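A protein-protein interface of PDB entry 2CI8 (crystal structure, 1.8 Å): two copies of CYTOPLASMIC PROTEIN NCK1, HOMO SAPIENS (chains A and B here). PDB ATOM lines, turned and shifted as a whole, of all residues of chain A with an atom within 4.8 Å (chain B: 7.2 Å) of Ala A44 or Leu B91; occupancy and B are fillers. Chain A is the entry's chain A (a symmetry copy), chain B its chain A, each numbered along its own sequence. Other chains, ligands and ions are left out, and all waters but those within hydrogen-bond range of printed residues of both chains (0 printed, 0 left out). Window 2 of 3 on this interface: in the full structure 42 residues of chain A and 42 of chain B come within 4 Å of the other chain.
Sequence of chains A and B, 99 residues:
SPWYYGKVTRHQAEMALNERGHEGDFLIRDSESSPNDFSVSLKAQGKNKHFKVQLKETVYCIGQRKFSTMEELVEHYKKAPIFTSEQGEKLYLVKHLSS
Of the 13 printed residues of chain B, 4 touch a printed residue of chain A. Hydrophobic or aromatic side chains of chain B within 4 Å of the printed part of chain A: Leu B91 and Leu B93. Among the printed residues, no Asp or Glu carboxylate lies within 4 Å of a Lys or Arg side-chain nitrogen of the other chain.
Of the printed residues of chain B, Ala A44 touches Leu B91 (3.996 Å). Of the printed residues of chain A, Leu B91 touches Ala A44 (3.996 Å), Gln A45 (3.8 Å) and Lys A49 (3.8 Å). Of the printed residues of chain A, Glu B89 touches Gln A45 (2.8 Å). Of the printed residues of chain B, Lys A49 touches Leu B91 (3.8 Å). Of the printed residues of chain A, Leu B93 touches Leu A42 (3.9 Å). Of the printed residues of chain A, Tyr B92 touches Leu A42 (3.96 Å). The nearest printed residue of chain A that does not touch Leu B91 is Leu A42 (4.4 Å).
The backbone carbonyl oxygen of Tyr B77 is in hydrogen-bond range of the backbone NH of Leu B93, at 3.0 Å. The backbone carbonyl oxygen (O) of Leu B91 sits at hydrogen-bond distance from the backbone NH (N) of Ile B82, 2.9 Å away. O of Phe B83 is in hydrogen-bond range of N of Leu B91 (2.8 Å). N of Glu B89 is in hydrogen-bond range of OG of Ser B85 (3.0 Å). The side-chain carboxylate of Glu A23 sits at hydrogen-bond distance from the backbone NH of Gln A45 (2.8 Å). O of Leu A42 is in hydrogen-bond range of N of Lys A49 (2.8 Å).
Among the printed residues, pairs that only touch across the chains: Lys A49 with Leu B91, Gln A45 with Leu B91, Leu A42 with Leu B93, Leu A42 with Tyr B92 and Ala A44 with Leu B91.
OE1 of Glu B89 sits at hydrogen-bond distance from NE2 of Gln A45 (2.8 Å).
No position is printed for both chains. Of the 6 pairs that touch across the chains among the printed residues, none has its exchanged pair printed and touching as well.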
ATOM      1  N   GLU A  23      17.538  14.721   0.687  1.00  0.00           N
ATOM      2  CA  GLU A  23      17.861  13.202   0.649  1.00  0.00           C
ATOM      3  C   GLU A  23      17.010  12.400   1.662  1.00  0.00           C
ATOM      4  O   GLU A  23      17.101  12.595   2.885  1.00  0.00           O
ATOM      5  CB  GLU A  23      19.376  12.927   0.997  1.00  0.00           C
ATOM      6  CG  GLU A  23      19.853  11.465   0.883  1.00  0.00           C
ATOM      7  CD  GLU A  23      20.287  11.071  -0.512  1.00  0.00           C
ATOM      8  OE1 GLU A  23      19.986  11.799  -1.461  1.00  0.00           O
ATOM      9  OE2 GLU A  23      20.962  10.013  -0.660  1.00  0.00           O
ATOM     10  N   LEU A  42      10.035  10.325  -3.834  1.00  0.00           N
ATOM     11  CA  LEU A  42      11.218  10.313  -2.983  1.00  0.00           C
ATOM     12  C   LEU A  42      12.291  11.159  -3.592  1.00  0.00           C
ATOM     13  O   LEU A  42      12.547  11.074  -4.773  1.00  0.00           O
ATOM     14  CB  LEU A  42      11.730   8.846  -2.856  1.00  0.00           C
ATOM     15  CG  LEU A  42      13.068   8.608  -2.111  1.00  0.00           C
ATOM     16  CD1 LEU A  42      12.916   8.977  -0.684  1.00  0.00           C
ATOM     17  CD2 LEU A  42      13.601   7.160  -2.262  1.00  0.00           C
ATOM     18  N   LYS A  43      12.978  11.956  -2.739  1.00  0.00           N
ATOM     19  CA  LYS A  43      14.158  12.701  -3.160  1.00  0.00           C
ATOM     20  C   LYS A  43      15.393  11.845  -2.742  1.00  0.00           C
ATOM     21  O   LYS A  43      15.491  11.482  -1.614  1.00  0.00           O
ATOM     22  CB  LYS A  43      14.204  14.054  -2.463  1.00  0.00           C
ATOM     23  CG  LYS A  43      15.376  14.915  -2.968  1.00  0.00           C
ATOM     24  CD  LYS A  43      15.266  16.323  -2.478  1.00  0.00           C
ATOM     25  CE  LYS A  43      16.297  17.250  -3.144  1.00  0.00           C
ATOM     26  NZ  LYS A  43      15.802  18.639  -3.182  1.00  0.00           N
ATOM     27  N   ALA A  44      16.224  11.502  -3.714  1.00  0.00           N
ATOM     28  CA  ALA A  44      17.416  10.669  -3.520  1.00  0.00           C
ATOM     29  C   ALA A  44      18.482  11.011  -4.591  1.00  0.00           C
ATOM     30  O   ALA A  44      18.173  11.080  -5.781  1.00  0.00           O
ATOM     31  CB  ALA A  44      17.040   9.187  -3.574  1.00  0.00           C
ATOM     32  N   GLN A  45      19.737  11.215  -4.185  1.00  0.00           N
ATOM     33  CA  GLN A  45      20.832  11.486  -5.148  1.00  0.00           C
ATOM     34  C   GLN A  45      20.610  12.767  -5.980  1.00  0.00           C
ATOM     35  O   GLN A  45      20.983  12.812  -7.160  1.00  0.00           O
ATOM     36  CB  GLN A  45      21.020  10.278  -6.107  1.00  0.00           C
ATOM     37  CG  GLN A  45      21.074   8.909  -5.410  1.00  0.00           C
ATOM     38  CD  GLN A  45      21.202   7.747  -6.381  1.00  0.00           C
ATOM     39  OE1 GLN A  45      20.387   7.580  -7.304  1.00  0.00           O
ATOM     40  NE2 GLN A  45      22.212   6.917  -6.161  1.00  0.00           N
ATOM     41  N   GLY A  46      20.003  13.803  -5.386  1.00  0.00           N
ATOM     42  CA  GLY A  46      19.674  15.012  -6.149  1.00  0.00           C
ATOM     43  C   GLY A  46      18.550  14.896  -7.180  1.00  0.00           C
ATOM     44  O   GLY A  46      18.322  15.840  -7.930  1.00  0.00           O
ATOM     45  N   LYS A  47      17.837  13.758  -7.192  1.00  0.00           N
ATOM     46  CA  LYS A  47      16.791  13.452  -8.197  1.00  0.00           C
ATOM     47  C   LYS A  47      15.512  13.043  -7.473  1.00  0.00           C
ATOM     48  O   LYS A  47      15.552  12.651  -6.315  1.00  0.00           O
ATOM     49  CB  LYS A  47      17.221  12.256  -9.062  1.00  0.00           C
ATOM     50  CG  LYS A  47      18.551  12.397  -9.791  1.00  0.00           C
ATOM     51  CD  LYS A  47      18.903  11.108 -10.545  1.00  0.00           C
ATOM     52  CE  LYS A  47      20.255  11.217 -11.290  1.00  0.00           C
ATOM     53  NZ  LYS A  47      20.552  10.012 -12.154  1.00  0.00           N
ATOM     54  N   LYS A  49      12.294  10.428  -7.473  1.00  0.00           N
ATOM     55  CA  LYS A  49      11.888   9.126  -7.987  1.00  0.00           C
ATOM     56  C   LYS A  49      10.465   8.871  -7.558  1.00  0.00           C
ATOM     57  O   LYS A  49      10.075   9.273  -6.461  1.00  0.00           O
ATOM     58  CB  LYS A  49      12.817   8.010  -7.526  1.00  0.00           C
ATOM     59  CG  LYS A  49      14.102   7.908  -8.403  1.00  0.00           C
ATOM     60  CD  LYS A  49      14.966   6.684  -8.128  1.00  0.00           C
ATOM     61  CE  LYS A  49      15.964   6.464  -9.276  1.00  0.00           C
ATOM     62  NZ  LYS A  49      16.722   7.732  -9.634  1.00  0.00           N
ATOM     63  N   TYR B  77      10.283   0.211   4.176  1.00  0.00           N
ATOM     64  CA  TYR B  77      11.202   0.842   3.274  1.00  0.00           C
ATOM     65  C   TYR B  77      12.156   1.889   3.861  1.00  0.00           C
ATOM     66  O   TYR B  77      12.971   2.462   3.129  1.00  0.00           O
ATOM     67  CB  TYR B  77      10.461   1.299   2.041  1.00  0.00           C
ATOM     68  CG  TYR B  77      10.011   0.106   1.242  1.00  0.00           C
ATOM     69  CD1 TYR B  77      10.943  -0.679   0.577  1.00  0.00           C
ATOM     70  CD2 TYR B  77       8.677  -0.238   1.134  1.00  0.00           C
ATOM     71  CE1 TYR B  77      10.553  -1.807  -0.186  1.00  0.00           C
ATOM     72  CE2 TYR B  77       8.279  -1.346   0.353  1.00  0.00           C
ATOM     73  CZ  TYR B  77       9.232  -2.122  -0.291  1.00  0.00           C
ATOM     74  OH  TYR B  77       8.864  -3.230  -1.049  1.00  0.00           O
ATOM     75  N   ALA B  80      14.605  -1.534   4.660  1.00  0.00           N
ATOM     76  CA  ALA B  80      15.005  -2.230   3.441  1.00  0.00           C
ATOM     77  C   ALA B  80      14.905  -1.231   2.301  1.00  0.00           C
ATOM     78  O   ALA B  80      14.116  -0.315   2.388  1.00  0.00           O
ATOM     79  CB  ALA B  80      14.098  -3.411   3.191  1.00  0.00           C
ATOM     80  N   PRO B  81      15.710  -1.386   1.248  1.00  0.00           N
ATOM     81  CA  PRO B  81      15.662  -0.428   0.158  1.00  0.00           C
ATOM     82  C   PRO B  81      14.409  -0.511  -0.724  1.00  0.00           C
ATOM     83  O   PRO B  81      13.943  -1.617  -1.090  1.00  0.00           O
ATOM     84  CB  PRO B  81      16.884  -0.785  -0.666  1.00  0.00           C
ATOM     85  CG  PRO B  81      17.099  -2.234  -0.402  1.00  0.00           C
ATOM     86  CD  PRO B  81      16.743  -2.415   1.017  1.00  0.00           C
ATOM     87  N   ILE B  82      13.891   0.651  -1.089  1.00  0.00           N
ATOM     88  CA  ILE B  82      12.699   0.727  -1.967  1.00  0.00           C
ATOM     89  C   ILE B  82      13.162   0.600  -3.426  1.00  0.00           C
ATOM     90  O   ILE B  82      12.374   0.261  -4.308  1.00  0.00           O
ATOM     91  CB  ILE B  82      11.934   2.028  -1.696  1.00  0.00           C
ATOM     92  CG1 ILE B  82      10.515   1.988  -2.285  1.00  0.00           C
ATOM     93  CG2 ILE B  82      12.708   3.178  -2.240  1.00  0.00           C
ATOM     94  CD1 ILE B  82       9.670   3.246  -1.940  1.00  0.00           C
ATOM     95  N   PHE B  83      14.455   0.861  -3.671  1.00  0.00           N
ATOM     96  CA  PHE B  83      15.084   0.725  -4.962  1.00  0.00           C
ATOM     97  C   PHE B  83      16.585   0.448  -4.775  1.00  0.00           C
ATOM     98  O   PHE B  83      17.264   1.097  -3.959  1.00  0.00           O
ATOM     99  CB  PHE B  83      14.936   1.999  -5.742  1.00  0.00           C
ATOM    100  CG  PHE B  83      15.532   1.953  -7.101  1.00  0.00           C
ATOM    101  CD1 PHE B  83      14.943   1.202  -8.097  1.00  0.00           C
ATOM    102  CD2 PHE B  83      16.671   2.686  -7.403  1.00  0.00           C
ATOM    103  CE1 PHE B  83      15.485   1.157  -9.369  1.00  0.00           C
ATOM    104  CE2 PHE B  83      17.218   2.655  -8.665  1.00  0.00           C
ATOM    105  CZ  PHE B  83      16.625   1.887  -9.656  1.00  0.00           C
ATOM    106  N   THR B  84      17.080  -0.520  -5.532  1.00  0.00           N
ATOM    107  CA  THR B  84      18.529  -0.797  -5.619  1.00  0.00           C
ATOM    108  C   THR B  84      18.886  -0.528  -7.059  1.00  0.00           C
ATOM    109  O   THR B  84      18.253  -1.077  -7.967  1.00  0.00           O
ATOM    110  CB  THR B  84      18.846  -2.231  -5.279  1.00  0.00           C
ATOM    111  OG1 THR B  84      18.356  -2.529  -3.968  1.00  0.00           O
ATOM    112  CG2 THR B  84      20.351  -2.465  -5.323  1.00  0.00           C
ATOM    113  N   SER B  85      19.854   0.339  -7.292  1.00  0.00           N
ATOM    114  CA  SER B  85      20.290   0.608  -8.650  1.00  0.00           C
ATOM    115  C   SER B  85      21.102  -0.589  -9.123  1.00  0.00           C
ATOM    116  O   SER B  85      21.374  -1.520  -8.358  1.00  0.00           O
ATOM    117  CB  SER B  85      21.168   1.856  -8.719  1.00  0.00           C
ATOM    118  OG  SER B  85      22.471   1.577  -8.245  1.00  0.00           O
ATOM    119  N   GLY B  88      24.267  -1.139  -7.433  1.00  0.00           N
ATOM    120  CA  GLY B  88      24.060  -1.658  -6.080  1.00  0.00           C
ATOM    121  C   GLY B  88      23.696  -0.592  -5.056  1.00  0.00           C
ATOM    122  O   GLY B  88      23.619  -0.881  -3.846  1.00  0.00           O
ATOM    123  N   GLU B  89      23.446   0.629  -5.538  1.00  0.00           N
ATOM    124  CA  GLU B  89      23.135   1.774  -4.678  1.00  0.00           C
ATOM    125  C   GLU B  89      21.734   1.597  -4.154  1.00  0.00           C
ATOM    126  O   GLU B  89      20.771   1.569  -4.943  1.00  0.00           O
ATOM    127  CB  GLU B  89      23.235   3.103  -5.456  1.00  0.00           C
ATOM    128  CG  GLU B  89      24.380   4.016  -5.005  1.00  0.00           C
ATOM    129  CD  GLU B  89      24.843   4.993  -6.091  1.00  0.00           C
ATOM    130  OE1 GLU B  89      24.175   5.116  -7.147  1.00  0.00           O
ATOM    131  OE2 GLU B  89      25.888   5.640  -5.877  1.00  0.00           O
ATOM    132  N   LYS B  90      21.633   1.439  -2.837  1.00  0.00           N
ATOM    133  CA  LYS B  90      20.380   1.241  -2.149  1.00  0.00           C
ATOM    134  C   LYS B  90      19.775   2.584  -1.725  1.00  0.00           C
ATOM    135  O   LYS B  90      20.435   3.372  -1.040  1.00  0.00           O
ATOM    136  CB  LYS B  90      20.600   0.402  -0.904  1.00  0.00           C
ATOM    137  CG  LYS B  90      21.131  -0.998  -1.180  1.00  0.00           C
ATOM    138  CD  LYS B  90      21.213  -1.806   0.109  1.00  0.00           C
ATOM    139  CE  LYS B  90      21.835  -3.174  -0.101  1.00  0.00           C
ATOM    140  NZ  LYS B  90      21.855  -3.962   1.179  1.00  0.00           N
ATOM    141  N   LEU B  91      18.525   2.821  -2.132  1.00  0.00           N
ATOM    142  CA  LEU B  91      17.784   4.033  -1.764  1.00  0.00           C
ATOM    143  C   LEU B  91      16.719   3.640  -0.755  1.00  0.00           C
ATOM    144  O   LEU B  91      15.999   2.673  -0.975  1.00  0.00           O
ATOM    145  CB  LEU B  91      17.122   4.639  -2.996  1.00  0.00           C
ATOM    146  CG  LEU B  91      17.997   4.838  -4.238  1.00  0.00           C
ATOM    147  CD1 LEU B  91      17.203   5.592  -5.312  1.00  0.00           C
ATOM    148  CD2 LEU B  91      19.298   5.590  -3.880  1.00  0.00           C
ATOM    149  N   TYR B  92      16.641   4.371   0.363  1.00  0.00           N
ATOM    150  CA  TYR B  92      15.701   4.141   1.422  1.00  0.00           C
ATOM    151  C   TYR B  92      14.858   5.396   1.643  1.00  0.00           C
ATOM    152  O   TYR B  92      15.272   6.495   1.299  1.00  0.00           O
ATOM    153  CB  TYR B  92      16.423   3.881   2.741  1.00  0.00           C
ATOM    154  CG  TYR B  92      17.397   2.727   2.723  1.00  0.00           C
ATOM    155  CD1 TYR B  92      18.638   2.861   2.117  1.00  0.00           C
ATOM    156  CD2 TYR B  92      17.095   1.530   3.333  1.00  0.00           C
ATOM    157  CE1 TYR B  92      19.538   1.811   2.097  1.00  0.00           C
ATOM    158  CE2 TYR B  92      18.005   0.478   3.333  1.00  0.00           C
ATOM    159  CZ  TYR B  92      19.203   0.620   2.709  1.00  0.00           C
ATOM    160  OH  TYR B  92      20.121  -0.423   2.693  1.00  0.00           O
ATOM    161  N   LEU B  93      13.688   5.194   2.228  1.00  0.00           N
ATOM    162  CA  LEU B  93      12.834   6.263   2.682  1.00  0.00           C
ATOM    163  C   LEU B  93      13.496   6.708   4.008  1.00  0.00           C
ATOM    164  O   LEU B  93      14.011   5.876   4.707  1.00  0.00           O
ATOM    165  CB  LEU B  93      11.429   5.756   2.992  1.00  0.00           C
ATOM    166  CG  LEU B  93      10.603   5.167   1.802  1.00  0.00           C
ATOM    167  CD1 LEU B  93       9.155   4.920   2.162  1.00  0.00           C
ATOM    168  CD2 LEU B  93      10.700   6.028   0.624  1.00  0.00           C
